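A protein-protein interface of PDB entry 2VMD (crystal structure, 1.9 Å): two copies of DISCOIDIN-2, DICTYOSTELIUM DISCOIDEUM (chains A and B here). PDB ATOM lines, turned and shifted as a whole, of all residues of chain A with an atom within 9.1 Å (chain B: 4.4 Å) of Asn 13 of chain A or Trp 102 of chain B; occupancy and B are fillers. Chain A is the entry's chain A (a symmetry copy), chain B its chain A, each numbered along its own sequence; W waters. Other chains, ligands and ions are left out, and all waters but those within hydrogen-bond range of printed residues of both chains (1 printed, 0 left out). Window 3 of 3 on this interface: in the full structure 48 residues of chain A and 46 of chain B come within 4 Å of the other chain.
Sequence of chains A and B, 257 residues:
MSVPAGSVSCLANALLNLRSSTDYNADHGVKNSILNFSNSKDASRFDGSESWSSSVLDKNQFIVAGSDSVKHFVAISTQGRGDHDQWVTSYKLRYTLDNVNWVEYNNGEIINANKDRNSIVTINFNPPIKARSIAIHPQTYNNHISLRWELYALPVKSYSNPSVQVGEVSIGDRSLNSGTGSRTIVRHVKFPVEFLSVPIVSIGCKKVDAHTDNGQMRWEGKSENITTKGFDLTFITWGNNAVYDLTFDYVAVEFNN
OG of Ser 133 of chain B lies within hydrogen-bond range of O of Asn 13 of chain A (2.7 Å). The side-chain amide oxygen (OD1) of Asn 13 of chain A lies close to the indole nitrogen (NE1) of Trp 102 of chain B, at 3.3 Å. ND2 of Asn 99 of chain B lies within hydrogen-bond range of OD1 of Asn 13 of chain A, 3.1 Å away. The backbone carbonyl oxygen (O) of Gly 66 of chain B sits close to the backbone carbonyl oxygen (O) of Ala 14 of chain A, at 3.3 Å.
ND2 of Asn 13 of chain A sits at hydrogen-bond distance from O of Ser 9 of chain A (2.7 Å). The side-chain hydroxyl (OG1) of Thr 96 of chain B is in hydrogen-bond range of the backbone NH (N) of Asn 99 of chain B, at 2.9 Å. The backbone NH of Leu 15 of chain A sits at hydrogen-bond distance from the backbone carbonyl oxygen of Cys 10 of chain A. The backbone NH (N) of Thr 96 of chain B lies within hydrogen-bond range of the backbone carbonyl oxygen (O) of Ser 133 of chain B (3.1 Å). OG1 of Thr 96 of chain B lies within hydrogen-bond range of O of Asn 101 of chain B (2.6 Å). The side-chain carboxylate of Glu 150 of chain A is in hydrogen-bond range of the backbone NH of Ala 12 of chain A (3.0 Å).
Among the printed residues, pairs that only touch across the chains: Ser 7 of chain A with Val 100 of chain B (3.9 Å), Val 8 of chain A with Asn 99 of chain B (3.7 Å), Val 8 of chain A with Val 100 of chain B (3.8 Å), Ala 12 of chain A with Val 64 of chain B (3.9 Å), Asn 13 of chain A with Val 64 of chain B (3.95 Å), Asn 13 of chain A with Gly 66 of chain B (3.9 Å), Asn 13 of chain A with Thr 96 of chain B (3.8 Å), Leu 15 of chain A with Asn 99 of chain B (3.7 Å) and Leu 15 of chain A with Ser 133 of chain B (3.9 Å).
Of the printed residues of chain B, Ser 7 of chain A touches Val 100. Of the printed residues of chain B, Ala 12 of chain A touches Val 64 (3.9 Å). Asn 13 of chain A touches just these residues of chain B: Val 64, Gly 66, Thr 96, Asn 99, Trp 102 and Ser 133. Of the printed residues of chain A, Val 64 of chain B touches Ala 12 (3.9 Å) and Asn 13 (3.95 Å). Asn 99 of chain B touches just these residues of chain A: Val 8, Asn 13 and Leu 15. Of chain A, only Asn 13 (3.3 Å) comes within 4 Å of Trp 102 of chain B. No residue of chain A comes within 4 Å of Val 103 of chain B. Printed residues of chain A within 4 Å of Ser 133 of chain B: Asn 13 and Leu 15. The nearest printed residue of chain B that does not touch Asn 13 of chain A is Val 100 of chain B (5.0 Å). The nearest printed residue of chain A that does not touch Ser 133 of chain B is Ala 14 of chain A (4.9 Å).
Of the 13 printed residues of chain B, 7 touch a printed residue of chain A. Hydrophobic or aromatic side chains of chain B within 4 Å of the printed part of chain A: Val 64, Val 100 and Trp 102. Along chain B the printed residues that touch a printed residue of chain A span positions 64 to 133. Of the 15 printed residues of chain A, 6 touch a printed residue of chain B. Among the printed residues, no Asp or Glu carboxylate lies within 4 Å of a Lys or Arg side-chain nitrogen of the other chain.
No position is printed for both chains. Of the 13 pairs that touch across the chains among the printed residues, none has its exchanged pair printed and touching as well.
Water W1 lies within hydrogen-bond range of O of Asn 99 of chain B (2.6 Å), N of Ser 9 of chain A (2.9 Å), ND2 of Asn 13 of chain A (3.3 Å) and O of Ser 7 of chain A (3.5 Å).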
ATOM      1  N   SER A   7     -22.634   6.220  28.201  1.00  0.00           N
ATOM      2  CA  SER A   7     -23.207   6.976  27.108  1.00  0.00           C
ATOM      3  C   SER A   7     -22.362   8.218  27.017  1.00  0.00           C
ATOM      4  O   SER A   7     -21.428   8.400  27.792  1.00  0.00           O
ATOM      5  CB  SER A   7     -24.671   7.303  27.388  1.00  0.00           C
ATOM      6  OG  SER A   7     -24.816   7.740  28.716  1.00  0.00           O
ATOM      7  N   VAL A   8     -22.672   9.072  26.063  1.00  0.00           N
ATOM      8  CA  VAL A   8     -21.905  10.286  25.866  1.00  0.00           C
ATOM      9  C   VAL A   8     -22.602  11.439  26.611  1.00  0.00           C
ATOM     10  O   VAL A   8     -23.795  11.606  26.497  1.00  0.00           O
ATOM     11  CB  VAL A   8     -21.809  10.585  24.362  1.00  0.00           C
ATOM     12  CG1 VAL A   8     -21.225  12.000  24.076  1.00  0.00           C
ATOM     13  CG2 VAL A   8     -21.006   9.459  23.661  1.00  0.00           C
ATOM     14  N   SER A   9     -21.838  12.201  27.394  1.00  0.00           N
ATOM     15  CA  SER A   9     -22.284  13.482  27.956  1.00  0.00           C
ATOM     16  C   SER A   9     -22.116  14.565  26.902  1.00  0.00           C
ATOM     17  O   SER A   9     -20.994  15.039  26.706  1.00  0.00           O
ATOM     18  CB  SER A   9     -21.353  13.833  29.124  1.00  0.00           C
ATOM     19  OG  SER A   9     -21.470  12.855  30.136  1.00  0.00           O
ATOM     20  N   CYS A  10     -23.187  14.953  26.218  1.00  0.00           N
ATOM     21  CA  CYS A  10     -23.043  15.782  25.004  1.00  0.00           C
ATOM     22  C   CYS A  10     -22.527  17.197  25.249  1.00  0.00           C
ATOM     23  O   CYS A  10     -21.689  17.693  24.493  1.00  0.00           O
ATOM     24  CB  CYS A  10     -24.346  15.887  24.227  1.00  0.00           C
ATOM     25  SG  CYS A  10     -25.098  14.302  23.705  1.00  0.00           S
ATOM     26  N   LEU A  11     -23.079  17.866  26.263  1.00  0.00           N
ATOM     27  CA  LEU A  11     -22.588  19.184  26.642  1.00  0.00           C
ATOM     28  C   LEU A  11     -21.161  19.129  27.193  1.00  0.00           C
ATOM     29  O   LEU A  11     -20.330  19.934  26.810  1.00  0.00           O
ATOM     30  CB  LEU A  11     -23.541  19.881  27.625  1.00  0.00           C
ATOM     31  CG  LEU A  11     -25.019  20.077  27.286  1.00  0.00           C
ATOM     32  CD1 LEU A  11     -25.552  21.268  28.076  1.00  0.00           C
ATOM     33  CD2 LEU A  11     -25.277  20.253  25.816  1.00  0.00           C
ATOM     34  N   ALA A  12     -20.850  18.176  28.070  1.00  0.00           N
ATOM     35  CA  ALA A  12     -19.474  18.080  28.576  1.00  0.00           C
ATOM     36  C   ALA A  12     -18.437  17.988  27.467  1.00  0.00           C
ATOM     37  O   ALA A  12     -17.324  18.522  27.586  1.00  0.00           O
ATOM     38  CB  ALA A  12     -19.302  16.880  29.545  1.00  0.00           C
ATOM     39  N   ASN A  13     -18.811  17.283  26.407  1.00  0.00           N
ATOM     40  CA  ASN A  13     -17.942  17.009  25.257  1.00  0.00           C
ATOM     41  C   ASN A  13     -18.024  18.076  24.178  1.00  0.00           C
ATOM     42  O   ASN A  13     -17.363  17.973  23.137  1.00  0.00           O
ATOM     43  CB  ASN A  13     -18.312  15.637  24.703  1.00  0.00           C
ATOM     44  CG  ASN A  13     -17.725  14.544  25.521  1.00  0.00           C
ATOM     45  OD1 ASN A  13     -16.611  14.162  25.290  1.00  0.00           O
ATOM     46  ND2 ASN A  13     -18.447  14.083  26.541  1.00  0.00           N
ATOM     47  N   ALA A  14     -18.800  19.127  24.454  1.00  0.00           N
ATOM     48  CA  ALA A  14     -19.052  20.242  23.500  1.00  0.00           C
ATOM     49  C   ALA A  14     -19.619  19.801  22.139  1.00  0.00           C
ATOM     50  O   ALA A  14     -19.255  20.332  21.071  1.00  0.00           O
ATOM     51  CB  ALA A  14     -17.820  21.086  23.330  1.00  0.00           C
ATOM     52  N   LEU A  15     -20.568  18.874  22.180  1.00  0.00           N
ATOM     53  CA  LEU A  15     -21.038  18.235  20.944  1.00  0.00           C
ATOM     54  C   LEU A  15     -22.241  18.939  20.335  1.00  0.00           C
ATOM     55  O   LEU A  15     -22.594  18.704  19.182  1.00  0.00           O
ATOM     56  CB  LEU A  15     -21.329  16.752  21.175  1.00  0.00           C
ATOM     57  CG  LEU A  15     -20.137  15.815  21.427  1.00  0.00           C
ATOM     58  CD1 LEU A  15     -20.641  14.386  21.692  1.00  0.00           C
ATOM     59  CD2 LEU A  15     -19.137  15.858  20.271  1.00  0.00           C
ATOM     60  N   LEU A  16     -22.888  19.802  21.111  1.00  0.00           N
ATOM     61  CA  LEU A  16     -24.120  20.417  20.667  1.00  0.00           C
ATOM     62  C   LEU A  16     -24.085  21.936  20.755  1.00  0.00           C
ATOM     63  O   LEU A  16     -23.595  22.474  21.726  1.00  0.00           O
ATOM     64  CB  LEU A  16     -25.287  19.893  21.511  1.00  0.00           C
ATOM     65  CG  LEU A  16     -25.556  18.384  21.544  1.00  0.00           C
ATOM     66  CD1 LEU A  16     -26.630  18.058  22.494  1.00  0.00           C
ATOM     67  CD2 LEU A  16     -25.920  17.855  20.178  1.00  0.00           C
ATOM     68  N   ILE A  34     -24.157  23.814  32.002  1.00  0.00           N
ATOM     69  CA  ILE A  34     -23.828  22.406  32.074  1.00  0.00           C
ATOM     70  C   ILE A  34     -24.069  21.887  33.466  1.00  0.00           C
ATOM     71  O   ILE A  34     -23.841  22.602  34.437  1.00  0.00           O
ATOM     72  CB  ILE A  34     -22.425  22.042  31.564  1.00  0.00           C
ATOM     73  CG1 ILE A  34     -22.383  20.524  31.270  1.00  0.00           C
ATOM     74  CG2 ILE A  34     -21.325  22.511  32.519  1.00  0.00           C
ATOM     75  CD1 ILE A  34     -21.037  19.990  30.858  1.00  0.00           C
ATOM     76  N   GLU A 150     -27.733  18.168  31.373  1.00  0.00           N
ATOM     77  CA  GLU A 150     -26.920  17.357  30.503  1.00  0.00           C
ATOM     78  C   GLU A 150     -27.814  16.439  29.645  1.00  0.00           C
ATOM     79  O   GLU A 150     -28.910  16.028  30.075  1.00  0.00           O
ATOM     80  CB  GLU A 150     -25.842  16.573  31.274  1.00  0.00           C
ATOM     81  CG  GLU A 150     -24.951  15.702  30.346  1.00  0.00           C
ATOM     82  CD  GLU A 150     -24.125  16.500  29.361  1.00  0.00           C
ATOM     83  OE1 GLU A 150     -22.943  16.767  29.659  1.00  0.00           O
ATOM     84  OE2 GLU A 150     -24.645  16.852  28.286  1.00  0.00           O
ATOM     85  N   LEU A 151     -27.383  16.220  28.402  1.00  0.00           N
ATOM     86  CA  LEU A 151     -28.055  15.303  27.502  1.00  0.00           C
ATOM     87  C   LEU A 151     -27.141  14.111  27.285  1.00  0.00           C
ATOM     88  O   LEU A 151     -25.965  14.300  27.065  1.00  0.00           O
ATOM     89  CB  LEU A 151     -28.343  15.971  26.174  1.00  0.00           C
ATOM     90  CG  LEU A 151     -29.472  16.987  26.183  1.00  0.00           C
ATOM     91  CD1 LEU A 151     -29.413  17.851  24.996  1.00  0.00           C
ATOM     92  CD2 LEU A 151     -30.819  16.239  26.157  1.00  0.00           C
ATOM     93  N   TYR A 152     -27.690  12.889  27.365  1.00  0.00           N
ATOM     94  CA  TYR A 152     -26.866  11.682  27.212  1.00  0.00           C
ATOM     95  C   TYR A 152     -27.292  10.929  25.981  1.00  0.00           C
ATOM     96  O   TYR A 152     -28.490  10.675  25.814  1.00  0.00           O
ATOM     97  CB  TYR A 152     -26.989  10.799  28.420  1.00  0.00           C
ATOM     98  CG  TYR A 152     -26.498  11.451  29.658  1.00  0.00           C
ATOM     99  CD1 TYR A 152     -25.142  11.389  30.012  1.00  0.00           C
ATOM    100  CD2 TYR A 152     -27.376  12.152  30.478  1.00  0.00           C
ATOM    101  CE1 TYR A 152     -24.685  12.016  31.162  1.00  0.00           C
ATOM    102  CE2 TYR A 152     -26.932  12.787  31.636  1.00  0.00           C
ATOM    103  CZ  TYR A 152     -25.583  12.693  31.981  1.00  0.00           C
ATOM    104  OH  TYR A 152     -25.126  13.311  33.121  1.00  0.00           O
ATOM    105  N   ALA A 153     -26.331  10.651  25.087  1.00  0.00           N
ATOM    106  CA  ALA A 153     -26.630   9.958  23.819  1.00  0.00           C
ATOM    107  C   ALA A 153     -25.810   8.676  23.711  1.00  0.00           C
ATOM    108  O   ALA A 153     -24.759   8.534  24.367  1.00  0.00           O
ATOM    109  CB  ALA A 153     -26.341  10.884  22.614  1.00  0.00           C
ATOM    110  N   VAL B  64     -12.904  23.022  26.282  1.00  0.00           N
ATOM    111  CA  VAL B  64     -13.159  21.877  25.403  1.00  0.00           C
ATOM    112  C   VAL B  64     -13.638  22.389  24.047  1.00  0.00           C
ATOM    113  O   VAL B  64     -14.480  23.283  23.992  1.00  0.00           O
ATOM    114  CB  VAL B  64     -14.301  20.972  25.937  1.00  0.00           C
ATOM    115  CG1 VAL B  64     -14.373  19.688  25.076  1.00  0.00           C
ATOM    116  CG2 VAL B  64     -14.067  20.642  27.385  1.00  0.00           C
ATOM    117  N   GLY B  66     -15.318  20.878  20.424  1.00  0.00           N
ATOM    118  CA  GLY B  66     -15.899  19.636  19.950  1.00  0.00           C
ATOM    119  C   GLY B  66     -16.813  19.778  18.770  1.00  0.00           C
ATOM    120  O   GLY B  66     -17.341  20.875  18.495  1.00  0.00           O
ATOM    121  N   ARG B  94      -5.849  17.002  26.425  1.00  0.00           N
ATOM    122  CA  ARG B  94      -6.519  15.700  26.561  1.00  0.00           C
ATOM    123  C   ARG B  94      -7.461  15.637  25.381  1.00  0.00           C
ATOM    124  O   ARG B  94      -7.937  16.685  24.923  1.00  0.00           O
ATOM    125  CB  ARG B  94      -7.438  15.624  27.785  1.00  0.00           C
ATOM    126  CG  ARG B  94      -7.070  16.316  29.011  1.00  0.00           C
ATOM    127  CD  ARG B  94      -8.161  16.058  29.998  1.00  0.00           C
ATOM    128  NE  ARG B  94      -8.284  14.652  30.344  1.00  0.00           N
ATOM    129  CZ  ARG B  94      -9.443  14.047  30.612  1.00  0.00           C
ATOM    130  NH1 ARG B  94     -10.602  14.710  30.558  1.00  0.00           N
ATOM    131  NH2 ARG B  94      -9.445  12.762  30.925  1.00  0.00           N
ATOM    132  N   TYR B  95      -7.798  14.438  24.928  1.00  0.00           N
ATOM    133  CA  TYR B  95      -8.727  14.326  23.808  1.00  0.00           C
ATOM    134  C   TYR B  95      -9.439  13.009  23.842  1.00  0.00           C
ATOM    135  O   TYR B  95      -9.072  12.115  24.600  1.00  0.00           O
ATOM    136  CB  TYR B  95      -8.024  14.509  22.445  1.00  0.00           C
ATOM    137  CG  TYR B  95      -6.984  13.456  22.133  1.00  0.00           C
ATOM    138  CD1 TYR B  95      -7.329  12.271  21.456  1.00  0.00           C
ATOM    139  CD2 TYR B  95      -5.662  13.638  22.507  1.00  0.00           C
ATOM    140  CE1 TYR B  95      -6.371  11.307  21.151  1.00  0.00           C
ATOM    141  CE2 TYR B  95      -4.697  12.677  22.224  1.00  0.00           C
ATOM    142  CZ  TYR B  95      -5.059  11.526  21.533  1.00  0.00           C
ATOM    143  OH  TYR B  95      -4.096  10.592  21.245  1.00  0.00           O
ATOM    144  N   THR B  96     -10.436  12.902  22.987  1.00  0.00           N
ATOM    145  CA  THR B  96     -11.309  11.742  22.911  1.00  0.00           C
ATOM    146  C   THR B  96     -11.818  11.547  21.477  1.00  0.00           C
ATOM    147  O   THR B  96     -12.168  12.500  20.772  1.00  0.00           O
ATOM    148  CB  THR B  96     -12.526  11.834  23.903  1.00  0.00           C
ATOM    149  OG1 THR B  96     -13.290  10.616  23.848  1.00  0.00           O
ATOM    150  CG2 THR B  96     -13.481  13.024  23.541  1.00  0.00           C
ATOM    151  N   ASN B  99     -15.892  10.088  22.655  1.00  0.00           N
ATOM    152  CA  ASN B  99     -16.581  10.982  23.592  1.00  0.00           C
ATOM    153  C   ASN B  99     -17.020  10.292  24.862  1.00  0.00           C
ATOM    154  O   ASN B  99     -17.964  10.730  25.533  1.00  0.00           O
ATOM    155  CB  ASN B  99     -17.742  11.688  22.911  1.00  0.00           C
ATOM    156  CG  ASN B  99     -17.286  12.659  21.842  1.00  0.00           C
ATOM    157  OD1 ASN B  99     -17.587  12.491  20.674  1.00  0.00           O
ATOM    158  ND2 ASN B  99     -16.587  13.696  22.241  1.00  0.00           N
ATOM    159  N   VAL B 100     -16.361   9.171  25.161  1.00  0.00           N
ATOM    160  CA  VAL B 100     -16.614   8.419  26.391  1.00  0.00           C
ATOM    161  C   VAL B 100     -15.280   8.259  27.109  1.00  0.00           C
ATOM    162  O   VAL B 100     -15.166   8.520  28.317  1.00  0.00           O
ATOM    163  CB  VAL B 100     -17.228   7.021  26.108  1.00  0.00           C
ATOM    164  CG1 VAL B 100     -17.314   6.192  27.388  1.00  0.00           C
ATOM    165  CG2 VAL B 100     -18.595   7.154  25.444  1.00  0.00           C
ATOM    166  N   ASN B 101     -14.278   7.877  26.330  1.00  0.00           N
ATOM    167  CA  ASN B 101     -12.926   7.624  26.808  1.00  0.00           C
ATOM    168  C   ASN B 101     -11.958   8.721  26.393  1.00  0.00           C
ATOM    169  O   ASN B 101     -11.753   8.973  25.206  1.00  0.00           O
ATOM    170  CB  ASN B 101     -12.460   6.247  26.329  1.00  0.00           C
ATOM    171  CG  ASN B 101     -13.308   5.116  26.921  1.00  0.00           C
ATOM    172  OD1 ASN B 101     -13.196   4.804  28.108  1.00  0.00           O
ATOM    173  ND2 ASN B 101     -14.205   4.550  26.108  1.00  0.00           N
ATOM    174  N   TRP B 102     -11.396   9.391  27.400  1.00  0.00           N
ATOM    175  CA  TRP B 102     -10.519  10.540  27.217  1.00  0.00           C
ATOM    176  C   TRP B 102      -9.082  10.105  27.401  1.00  0.00           C
ATOM    177  O   TRP B 102      -8.791   9.266  28.264  1.00  0.00           O
ATOM    178  CB  TRP B 102     -10.860  11.659  28.211  1.00  0.00           C
ATOM    179  CG  TRP B 102     -12.015  12.457  27.758  1.00  0.00           C
ATOM    180  CD1 TRP B 102     -13.335  12.110  27.829  1.00  0.00           C
ATOM    181  CD2 TRP B 102     -11.962  13.707  27.091  1.00  0.00           C
ATOM    182  NE1 TRP B 102     -14.120  13.084  27.243  1.00  0.00           N
ATOM    183  CE2 TRP B 102     -13.292  14.077  26.783  1.00  0.00           C
ATOM    184  CE3 TRP B 102     -10.913  14.562  26.715  1.00  0.00           C
ATOM    185  CZ2 TRP B 102     -13.599  15.270  26.123  1.00  0.00           C
ATOM    186  CZ3 TRP B 102     -11.218  15.738  26.077  1.00  0.00           C
ATOM    187  CH2 TRP B 102     -12.556  16.085  25.783  1.00  0.00           C
ATOM    188  N   VAL B 103      -8.199  10.623  26.567  1.00  0.00           N
ATOM    189  CA  VAL B 103      -6.786  10.307  26.730  1.00  0.00           C
ATOM    190  C   VAL B 103      -5.949  11.556  26.901  1.00  0.00           C
ATOM    191  O   VAL B 103      -6.313  12.627  26.431  1.00  0.00           O
ATOM    192  CB  VAL B 103      -6.200   9.419  25.607  1.00  0.00           C
ATOM    193  CG1 VAL B 103      -6.964   8.089  25.516  1.00  0.00           C
ATOM    194  CG2 VAL B 103      -6.153  10.121  24.304  1.00  0.00           C
ATOM    195  N   SER B 133     -13.387  15.563  20.202  1.00  0.00           N
ATOM    196  CA  SER B 133     -13.257  16.681  21.138  1.00  0.00           C
ATOM    197  C   SER B 133     -11.851  16.677  21.711  1.00  0.00           C
ATOM    198  O   SER B 133     -11.237  15.621  21.856  1.00  0.00           O
ATOM    199  CB  SER B 133     -14.239  16.547  22.310  1.00  0.00           C
ATOM    200  OG  SER B 133     -15.587  16.481  21.844  1.00  0.00           O
ATOM    201  N   ILE B 134     -11.387  17.864  22.076  1.00  0.00           N
ATOM    202  CA  ILE B 134     -10.052  18.077  22.538  1.00  0.00           C
ATOM    203  C   ILE B 134     -10.143  19.201  23.555  1.00  0.00           C
ATOM    204  O   ILE B 134     -10.998  20.075  23.416  1.00  0.00           O
ATOM    205  CB  ILE B 134      -9.088  18.428  21.360  1.00  0.00           C
ATOM    206  CG1 ILE B 134      -7.661  18.634  21.882  1.00  0.00           C
ATOM    207  CG2 ILE B 134      -9.580  19.653  20.599  1.00  0.00           C
ATOM    208  CD1 ILE B 134      -6.576  18.369  20.846  1.00  0.00           C
ATOM    209  N   ALA B 135      -9.301  19.152  24.587  1.00  0.00           N
ATOM    210  CA  ALA B 135      -9.373  20.125  25.685  1.00  0.00           C
ATOM    211  C   ALA B 135      -7.986  20.621  25.981  1.00  0.00           C
ATOM    212  O   ALA B 135      -7.037  19.825  26.093  1.00  0.00           O
ATOM    213  CB  ALA B 135      -9.964  19.499  26.950  1.00  0.00           C
HETATM  214  O   HOH W   1     -19.230  11.089  27.803  1.00  0.00           O
